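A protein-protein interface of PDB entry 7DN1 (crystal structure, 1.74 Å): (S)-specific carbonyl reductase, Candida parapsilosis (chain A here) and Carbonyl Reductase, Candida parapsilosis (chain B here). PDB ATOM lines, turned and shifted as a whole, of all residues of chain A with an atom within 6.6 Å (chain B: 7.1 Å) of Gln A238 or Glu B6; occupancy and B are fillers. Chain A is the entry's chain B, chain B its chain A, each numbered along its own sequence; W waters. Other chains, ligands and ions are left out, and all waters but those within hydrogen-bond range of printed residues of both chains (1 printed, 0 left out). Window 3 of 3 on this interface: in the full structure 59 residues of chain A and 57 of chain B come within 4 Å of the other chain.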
ATOM      1  N   ASP A 231      36.636   5.875  -2.501  1.00  0.00           N
ATOM      2  CA  ASP A 231      36.142   5.432  -1.205  1.00  0.00           C
ATOM      3  C   ASP A 231      35.022   6.330  -0.700  1.00  0.00           C
ATOM      4  O   ASP A 231      34.153   5.863   0.042  1.00  0.00           O
ATOM      5  CB  ASP A 231      37.278   5.403  -0.183  1.00  0.00           C
ATOM      6  CG  ASP A 231      38.186   4.178  -0.338  1.00  0.00           C
ATOM      7  OD1 ASP A 231      37.742   3.139  -0.872  1.00  0.00           O
ATOM      8  OD2 ASP A 231      39.358   4.271   0.062  1.00  0.00           O
ATOM      9  N   LYS A 233      32.736   8.049  -2.771  1.00  0.00           N
ATOM     10  CA  LYS A 233      31.571   7.672  -3.568  1.00  0.00           C
ATOM     11  C   LYS A 233      30.989   6.346  -3.113  1.00  0.00           C
ATOM     12  O   LYS A 233      29.764   6.172  -3.083  1.00  0.00           O
ATOM     13  CB  LYS A 233      31.954   7.568  -5.041  1.00  0.00           C
ATOM     14  CG  LYS A 233      32.102   8.868  -5.776  1.00  0.00           C
ATOM     15  CD  LYS A 233      32.553   8.557  -7.186  1.00  0.00           C
ATOM     16  CE  LYS A 233      32.697   9.791  -8.038  1.00  0.00           C
ATOM     17  NZ  LYS A 233      33.149   9.395  -9.408  1.00  0.00           N
ATOM     18  N   ALA A 234      31.858   5.382  -2.795  1.00  0.00           N
ATOM     19  CA  ALA A 234      31.385   4.063  -2.390  1.00  0.00           C
ATOM     20  C   ALA A 234      30.506   4.159  -1.152  1.00  0.00           C
ATOM     21  O   ALA A 234      29.504   3.446  -1.033  1.00  0.00           O
ATOM     22  CB  ALA A 234      32.566   3.134  -2.132  1.00  0.00           C
ATOM     23  N   LYS A 235      30.874   5.032  -0.216  1.00  0.00           N
ATOM     24  CA  LYS A 235      30.042   5.242   0.961  1.00  0.00           C
ATOM     25  C   LYS A 235      28.702   5.885   0.600  1.00  0.00           C
ATOM     26  O   LYS A 235      27.668   5.519   1.166  1.00  0.00           O
ATOM     27  CB  LYS A 235      30.817   6.070   1.986  1.00  0.00           C
ATOM     28  CG  LYS A 235      32.050   5.335   2.504  1.00  0.00           C
ATOM     29  CD  LYS A 235      32.583   5.982   3.787  1.00  0.00           C
ATOM     30  CE  LYS A 235      33.811   5.251   4.320  1.00  0.00           C
ATOM     31  NZ  LYS A 235      35.057   5.398   3.488  1.00  0.00           N
ATOM     32  N   TRP A 236      28.684   6.828  -0.354  1.00  0.00           N
ATOM     33  CA  TRP A 236      27.405   7.369  -0.811  1.00  0.00           C
ATOM     34  C   TRP A 236      26.510   6.262  -1.356  1.00  0.00           C
ATOM     35  O   TRP A 236      25.317   6.201  -1.025  1.00  0.00           O
ATOM     36  CB  TRP A 236      27.612   8.446  -1.875  1.00  0.00           C
ATOM     37  CG  TRP A 236      28.425   9.610  -1.449  1.00  0.00           C
ATOM     38  CD1 TRP A 236      28.688  10.010  -0.170  1.00  0.00           C
ATOM     39  CD2 TRP A 236      29.069  10.552  -2.310  1.00  0.00           C
ATOM     40  NE1 TRP A 236      29.482  11.139  -0.186  1.00  0.00           N
ATOM     41  CE2 TRP A 236      29.724  11.492  -1.490  1.00  0.00           C
ATOM     42  CE3 TRP A 236      29.160  10.688  -3.702  1.00  0.00           C
ATOM     43  CZ2 TRP A 236      30.467  12.548  -2.014  1.00  0.00           C
ATOM     44  CZ3 TRP A 236      29.900  11.737  -4.218  1.00  0.00           C
ATOM     45  CH2 TRP A 236      30.544  12.652  -3.379  1.00  0.00           C
ATOM     46  N   TRP A 237      27.071   5.389  -2.204  1.00  0.00           N
ATOM     47  CA  TRP A 237      26.296   4.291  -2.787  1.00  0.00           C
ATOM     48  C   TRP A 237      25.723   3.383  -1.708  1.00  0.00           C
ATOM     49  O   TRP A 237      24.580   2.918  -1.819  1.00  0.00           O
ATOM     50  CB  TRP A 237      27.162   3.450  -3.733  1.00  0.00           C
ATOM     51  CG  TRP A 237      27.840   4.186  -4.860  1.00  0.00           C
ATOM     52  CD1 TRP A 237      27.447   5.357  -5.446  1.00  0.00           C
ATOM     53  CD2 TRP A 237      29.052   3.796  -5.508  1.00  0.00           C
ATOM     54  NE1 TRP A 237      28.332   5.697  -6.453  1.00  0.00           N
ATOM     55  CE2 TRP A 237      29.333   4.764  -6.497  1.00  0.00           C
ATOM     56  CE3 TRP A 237      29.917   2.710  -5.359  1.00  0.00           C
ATOM     57  CZ2 TRP A 237      30.454   4.672  -7.336  1.00  0.00           C
ATOM     58  CZ3 TRP A 237      31.034   2.628  -6.184  1.00  0.00           C
ATOM     59  CH2 TRP A 237      31.287   3.607  -7.156  1.00  0.00           C
ATOM     60  N   GLN A 238      26.530   3.074  -0.682  1.00  0.00           N
ATOM     61  CA  GLN A 238      26.093   2.174   0.385  1.00  0.00           C
ATOM     62  C   GLN A 238      24.897   2.720   1.156  1.00  0.00           C
ATOM     63  O   GLN A 238      24.123   1.940   1.727  1.00  0.00           O
ATOM     64  CB  GLN A 238      27.227   1.923   1.364  1.00  0.00           C
ATOM     65  CG  GLN A 238      28.353   1.060   0.808  1.00  0.00           C
ATOM     66  CD  GLN A 238      29.402   0.852   1.855  1.00  0.00           C
ATOM     67  OE1 GLN A 238      29.916   1.820   2.425  1.00  0.00           O
ATOM     68  NE2 GLN A 238      29.713  -0.404   2.143  1.00  0.00           N
ATOM     69  N   LEU A 239      24.762   4.039   1.229  1.00  0.00           N
ATOM     70  CA  LEU A 239      23.684   4.687   1.962  1.00  0.00           C
ATOM     71  C   LEU A 239      22.530   5.124   1.067  1.00  0.00           C
ATOM     72  O   LEU A 239      21.562   5.693   1.577  1.00  0.00           O
ATOM     73  CB  LEU A 239      24.252   5.880   2.740  1.00  0.00           C
ATOM     74  CG  LEU A 239      24.761   5.517   4.149  1.00  0.00           C
ATOM     75  CD1 LEU A 239      25.984   4.685   4.114  1.00  0.00           C
ATOM     76  CD2 LEU A 239      25.108   6.795   4.877  1.00  0.00           C
ATOM     77  N   THR A 240      22.605   4.857  -0.247  1.00  0.00           N
ATOM     78  CA  THR A 240      21.540   5.210  -1.181  1.00  0.00           C
ATOM     79  C   THR A 240      20.682   3.990  -1.462  1.00  0.00           C
ATOM     80  O   THR A 240      21.203   2.988  -1.961  1.00  0.00           O
ATOM     81  CB  THR A 240      22.122   5.739  -2.490  1.00  0.00           C
ATOM     82  OG1 THR A 240      22.965   6.871  -2.217  1.00  0.00           O
ATOM     83  CG2 THR A 240      20.979   6.141  -3.461  1.00  0.00           C
ATOM     84  N   PRO A 241      19.378   4.034  -1.189  1.00  0.00           N
ATOM     85  CA  PRO A 241      18.530   2.841  -1.388  1.00  0.00           C
ATOM     86  C   PRO A 241      18.552   2.266  -2.791  1.00  0.00           C
ATOM     87  O   PRO A 241      18.516   1.034  -2.931  1.00  0.00           O
ATOM     88  CB  PRO A 241      17.141   3.354  -0.985  1.00  0.00           C
ATOM     89  CG  PRO A 241      17.463   4.390   0.027  1.00  0.00           C
ATOM     90  CD  PRO A 241      18.720   5.054  -0.362  1.00  0.00           C
ATOM     91  N   GLY A 243      21.197   2.371  -4.685  1.00  0.00           N
ATOM     92  CA  GLY A 243      22.519   1.768  -4.817  1.00  0.00           C
ATOM     93  C   GLY A 243      23.431   2.425  -5.824  1.00  0.00           C
ATOM     94  O   GLY A 243      24.415   1.802  -6.241  1.00  0.00           O
ATOM     95  N   ARG A 244      23.153   3.663  -6.219  1.00  0.00           N
ATOM     96  CA  ARG A 244      23.919   4.284  -7.291  1.00  0.00           C
ATOM     97  C   ARG A 244      23.695   5.787  -7.248  1.00  0.00           C
ATOM     98  O   ARG A 244      22.780   6.283  -6.582  1.00  0.00           O
ATOM     99  CB  ARG A 244      23.499   3.731  -8.647  1.00  0.00           C
ATOM    100  CG  ARG A 244      22.024   3.995  -8.963  1.00  0.00           C
ATOM    101  CD  ARG A 244      21.692   3.510 -10.370  1.00  0.00           C
ATOM    102  NE  ARG A 244      20.259   3.648 -10.637  1.00  0.00           N
ATOM    103  CZ  ARG A 244      19.697   4.752 -11.117  1.00  0.00           C
ATOM    104  NH1 ARG A 244      20.446   5.818 -11.371  1.00  0.00           N
ATOM    105  NH2 ARG A 244      18.386   4.797 -11.341  1.00  0.00           N
ATOM    106  N   SER B   1      31.768 -12.171  -0.072  1.00  0.00           N
ATOM    107  CA  SER B   1      31.523 -10.749   0.113  1.00  0.00           C
ATOM    108  C   SER B   1      32.798  -9.906   0.013  1.00  0.00           C
ATOM    109  O   SER B   1      32.721  -8.713  -0.299  1.00  0.00           O
ATOM    110  CB  SER B   1      30.829 -10.498   1.455  1.00  0.00           C
ATOM    111  OG  SER B   1      29.435 -10.746   1.355  1.00  0.00           O
ATOM    112  N   GLU B   4      33.428  -6.947  -2.853  1.00  0.00           N
ATOM    113  CA  GLU B   4      32.149  -6.326  -3.165  1.00  0.00           C
ATOM    114  C   GLU B   4      31.932  -5.149  -2.236  1.00  0.00           C
ATOM    115  O   GLU B   4      32.261  -5.216  -1.047  1.00  0.00           O
ATOM    116  CB  GLU B   4      30.987  -7.317  -3.017  1.00  0.00           C
ATOM    117  CG  GLU B   4      30.987  -8.394  -4.117  1.00  0.00           C
ATOM    118  CD  GLU B   4      30.561  -9.753  -3.600  1.00  0.00           C
ATOM    119  OE1 GLU B   4      31.090 -10.780  -4.087  1.00  0.00           O
ATOM    120  OE2 GLU B   4      29.693  -9.786  -2.698  1.00  0.00           O
ATOM    121  N   ILE B   5      31.362  -4.076  -2.775  1.00  0.00           N
ATOM    122  CA  ILE B   5      30.803  -3.016  -1.945  1.00  0.00           C
ATOM    123  C   ILE B   5      29.376  -3.430  -1.618  1.00  0.00           C
ATOM    124  O   ILE B   5      28.527  -3.514  -2.510  1.00  0.00           O
ATOM    125  CB  ILE B   5      30.840  -1.655  -2.646  1.00  0.00           C
ATOM    126  CG1 ILE B   5      32.273  -1.225  -2.949  1.00  0.00           C
ATOM    127  CG2 ILE B   5      30.157  -0.592  -1.782  1.00  0.00           C
ATOM    128  CD1 ILE B   5      32.378  -0.179  -4.040  1.00  0.00           C
ATOM    129  N   GLU B   6      29.108  -3.701  -0.340  1.00  0.00           N
ATOM    130  CA  GLU B   6      27.803  -4.173   0.101  1.00  0.00           C
ATOM    131  C   GLU B   6      26.971  -3.005   0.608  1.00  0.00           C
ATOM    132  O   GLU B   6      27.456  -2.194   1.407  1.00  0.00           O
ATOM    133  CB  GLU B   6      27.921  -5.216   1.213  1.00  0.00           C
ATOM    134  CG  GLU B   6      26.572  -5.881   1.486  1.00  0.00           C
ATOM    135  CD  GLU B   6      26.615  -6.946   2.560  1.00  0.00           C
ATOM    136  OE1 GLU B   6      27.251  -7.994   2.333  1.00  0.00           O
ATOM    137  OE2 GLU B   6      25.981  -6.738   3.624  1.00  0.00           O
ATOM    138  N   SER B   7      25.717  -2.938   0.167  1.00  0.00           N
ATOM    139  CA  SER B   7      24.828  -1.863   0.604  1.00  0.00           C
ATOM    140  C   SER B   7      24.614  -1.949   2.110  1.00  0.00           C
ATOM    141  O   SER B   7      24.503  -3.041   2.676  1.00  0.00           O
ATOM    142  CB  SER B   7      23.478  -1.952  -0.122  1.00  0.00           C
ATOM    143  OG  SER B   7      22.482  -1.069   0.427  1.00  0.00           O
ATOM    144  N   TYR B   8      24.561  -0.782   2.757  1.00  0.00           N
ATOM    145  CA  TYR B   8      24.035  -0.697   4.113  1.00  0.00           C
ATOM    146  C   TYR B   8      22.505  -0.714   4.144  1.00  0.00           C
ATOM    147  O   TYR B   8      21.927  -1.061   5.181  1.00  0.00           O
ATOM    148  CB  TYR B   8      24.572   0.566   4.795  1.00  0.00           C
ATOM    149  CG  TYR B   8      25.939   0.404   5.437  1.00  0.00           C
ATOM    150  CD1 TYR B   8      26.939  -0.336   4.819  1.00  0.00           C
ATOM    151  CD2 TYR B   8      26.227   0.994   6.664  1.00  0.00           C
ATOM    152  CE1 TYR B   8      28.182  -0.486   5.408  1.00  0.00           C
ATOM    153  CE2 TYR B   8      27.459   0.843   7.264  1.00  0.00           C
ATOM    154  CZ  TYR B   8      28.442   0.093   6.629  1.00  0.00           C
ATOM    155  OH  TYR B   8      29.701  -0.075   7.193  1.00  0.00           O
ATOM    156  N   CYS B   9      21.836  -0.361   3.038  1.00  0.00           N
ATOM    157  CA  CYS B   9      20.371  -0.368   3.000  1.00  0.00           C
ATOM    158  C   CYS B   9      19.797  -1.748   2.694  1.00  0.00           C
ATOM    159  O   CYS B   9      18.900  -2.223   3.397  1.00  0.00           O
ATOM    160  CB  CYS B   9      19.829   0.647   1.972  1.00  0.00           C
ATOM    161  SG  CYS B   9      20.471   2.328   2.122  1.00  0.00           S
ATOM    162  N   ASN B  10      20.287  -2.408   1.643  1.00  0.00           N
ATOM    163  CA  ASN B  10      19.633  -3.630   1.174  1.00  0.00           C
ATOM    164  C   ASN B  10      20.670  -4.450   0.406  1.00  0.00           C
ATOM    165  O   ASN B  10      20.959  -4.149  -0.755  1.00  0.00           O
ATOM    166  CB  ASN B  10      18.427  -3.298   0.310  1.00  0.00           C
ATOM    167  CG  ASN B  10      17.521  -4.486   0.081  1.00  0.00           C
ATOM    168  OD1 ASN B  10      17.939  -5.629   0.216  1.00  0.00           O
ATOM    169  ND2 ASN B  10      16.261  -4.216  -0.294  1.00  0.00           N
ATOM    170  N   LYS B  11      21.196  -5.490   1.052  1.00  0.00           N
ATOM    171  CA  LYS B  11      22.219  -6.305   0.407  1.00  0.00           C
ATOM    172  C   LYS B  11      21.684  -7.028  -0.822  1.00  0.00           C
ATOM    173  O   LYS B  11      22.471  -7.501  -1.653  1.00  0.00           O
ATOM    174  CB  LYS B  11      22.785  -7.294   1.421  1.00  0.00           C
ATOM    175  CG  LYS B  11      21.862  -8.454   1.697  1.00  0.00           C
ATOM    176  CD  LYS B  11      22.573  -9.539   2.504  1.00  0.00           C
ATOM    177  CE  LYS B  11      21.673 -10.755   2.641  1.00  0.00           C
ATOM    178  NZ  LYS B  11      20.553 -10.482   3.595  1.00  0.00           N
ATOM    179  N   GLU B  12      20.366  -7.112  -0.979  1.00  0.00           N
ATOM    180  CA  GLU B  12      19.855  -7.749  -2.184  1.00  0.00           C
ATOM    181  C   GLU B  12      20.009  -6.871  -3.422  1.00  0.00           C
ATOM    182  O   GLU B  12      19.685  -7.331  -4.525  1.00  0.00           O
ATOM    183  CB  GLU B  12      18.398  -8.162  -1.974  1.00  0.00           C
ATOM    184  CG  GLU B  12      18.273  -9.532  -1.308  1.00  0.00           C
ATOM    185  CD  GLU B  12      18.618 -10.684  -2.250  1.00  0.00           C
ATOM    186  OE1 GLU B  12      17.804 -10.984  -3.154  1.00  0.00           O
ATOM    187  OE2 GLU B  12      19.703 -11.292  -2.085  1.00  0.00           O
ATOM    188  N   LEU B  13      20.510  -5.638  -3.281  1.00  0.00           N
ATOM    189  CA  LEU B  13      20.923  -4.869  -4.452  1.00  0.00           C
ATOM    190  C   LEU B  13      22.090  -5.511  -5.183  1.00  0.00           C
ATOM    191  O   LEU B  13      22.282  -5.235  -6.375  1.00  0.00           O
ATOM    192  CB  LEU B  13      21.327  -3.445  -4.078  1.00  0.00           C
ATOM    193  CG  LEU B  13      20.235  -2.516  -3.538  1.00  0.00           C
ATOM    194  CD1 LEU B  13      20.848  -1.370  -2.740  1.00  0.00           C
ATOM    195  CD2 LEU B  13      19.425  -1.998  -4.733  1.00  0.00           C
ATOM    196  N   GLY B  14      22.876  -6.338  -4.500  1.00  0.00           N
ATOM    197  CA  GLY B  14      24.060  -6.912  -5.087  1.00  0.00           C
ATOM    198  C   GLY B  14      25.233  -5.967  -4.953  1.00  0.00           C
ATOM    199  O   GLY B  14      25.140  -4.923  -4.309  1.00  0.00           O
ATOM    200  N   PRO B  15      26.375  -6.335  -5.535  1.00  0.00           N
ATOM    201  CA  PRO B  15      27.568  -5.488  -5.428  1.00  0.00           C
ATOM    202  C   PRO B  15      27.333  -4.118  -6.046  1.00  0.00           C
ATOM    203  O   PRO B  15      26.779  -3.994  -7.140  1.00  0.00           O
ATOM    204  CB  PRO B  15      28.623  -6.272  -6.212  1.00  0.00           C
ATOM    205  CG  PRO B  15      28.135  -7.690  -6.193  1.00  0.00           C
ATOM    206  CD  PRO B  15      26.638  -7.567  -6.289  1.00  0.00           C
ATOM    207  N   LEU B  16      27.789  -3.103  -5.359  1.00  0.00           N
ATOM    208  CA  LEU B  16      27.509  -1.738  -5.764  1.00  0.00           C
ATOM    209  C   LEU B  16      28.634  -1.178  -6.627  1.00  0.00           C
ATOM    210  O   LEU B  16      29.771  -1.662  -6.574  1.00  0.00           O
ATOM    211  CB  LEU B  16      27.309  -0.851  -4.529  1.00  0.00           C
ATOM    212  CG  LEU B  16      26.168  -1.270  -3.596  1.00  0.00           C
ATOM    213  CD1 LEU B  16      26.053  -0.251  -2.480  1.00  0.00           C
ATOM    214  CD2 LEU B  16      24.824  -1.415  -4.353  1.00  0.00           C
HETATM  215  O   HOH W   1      22.807   0.916  -1.369  1.00  0.00           O
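The backbone carbonyl oxygen (O) of Glu B6 sits at hydrogen-bond distance from the side-chain amide nitrogen (NE2) of Gln A238 (3.0 Å). N of Tyr B8 is in hydrogen-bond range of O of Gln A238, 2.9 Å away. The side-chain sulfur of Cys B9 sits at hydrogen-bond distance from the backbone carbonyl oxygen of Leu A239, 3.6 Å away. The backbone carbonyl oxygen of Gln A238 lies within hydrogen-bond range of the backbone NH of Cys B9, 3.5 Å away.
The side-chain hydroxyl of Ser B7 lies within hydrogen-bond range of the backbone NH of Asn B10, at 2.8 Å. OG of Ser B7 sits at hydrogen-bond distance from N of Cys B9 (2.8 Å). The backbone carbonyl oxygen of Ile B5 lies within hydrogen-bond range of the backbone NH of Leu B16, at 3.0 Å. The backbone carbonyl oxygen of Trp A236 lies within hydrogen-bond range of the side-chain hydroxyl of Thr A240 (2.7 Å).
CB of Ala A234 touches CD1 of Ile B5, 3.8 Å away. Ile B5 touches Trp A237. O of Trp A237 touches CD1 of Leu B16 (3.6 Å). Gln A238 touches Ile B5. Gln A238 touches Ser B7 (O to OG, 3.7 Å). Leu B16 touches Gln A238 (CD1 to CA, 3.8 Å). C of Thr A240 touches SG of Cys B9 (3.96 Å). Pro A241 touches Cys B9 (N to SG, 3.9 Å). Leu B13 touches Pro A241 (CD1 to O, 3.4 Å). Gly A243 touches Leu B16 (O to CD2, 3.8 Å).
Printed residues of chain B within 4 Å of Ala A234: Ile B5. Of the printed residues of chain B, Gln A238 touches Ile B5 (3.6 Å), Glu B6 (3.0 Å), Ser B7 (3.7 Å), Tyr B8 (2.9 Å), Cys B9 (3.5 Å) and Leu B16 (3.8 Å). Of the printed residues of chain B, Thr A240 touches Cys B9 (3.96 Å). Ser B1 touches none of the printed residues of chain A. Glu B4 touches none of the printed residues of chain A. Of the printed residues of chain A, Ile B5 touches Ala A234, Trp A237 and Gln A238. Of chain A, only Gln A238 (3.0 Å) comes within 4 Å of Glu B6. Printed residues of chain A within 4 Å of Ser B7: Gln A238. Of the printed residues of chain A, Tyr B8 touches Gln A238. The nearest printed residue of chain B that does not touch Trp A237 is Ser B7 (5.0 Å).
Of the 14 printed residues of chain B, 7 touch a printed residue of chain A. Printed residues of chain B that touch a printed residue of chain A: Ile B5, Glu B6, Ser B7, Tyr B8, Cys B9, Leu B13 and Leu B16. Hydrophobic or aromatic side chains of chain B within 4 Å of the printed part of chain A: Ile B5, Tyr B8, Leu B13 and Leu B16. Of the 12 printed residues of chain A, 7 touch a printed residue of chain B. Hydrophobic or aromatic side chains of chain A within 4 Å of the printed part of chain B: Ala A234 and Trp A237.
Water W1 lies within hydrogen-bond range of O of Thr A240 (2.7 Å), OG of Ser B7 (2.7 Å) and O of Trp A237 (2.7 Å).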
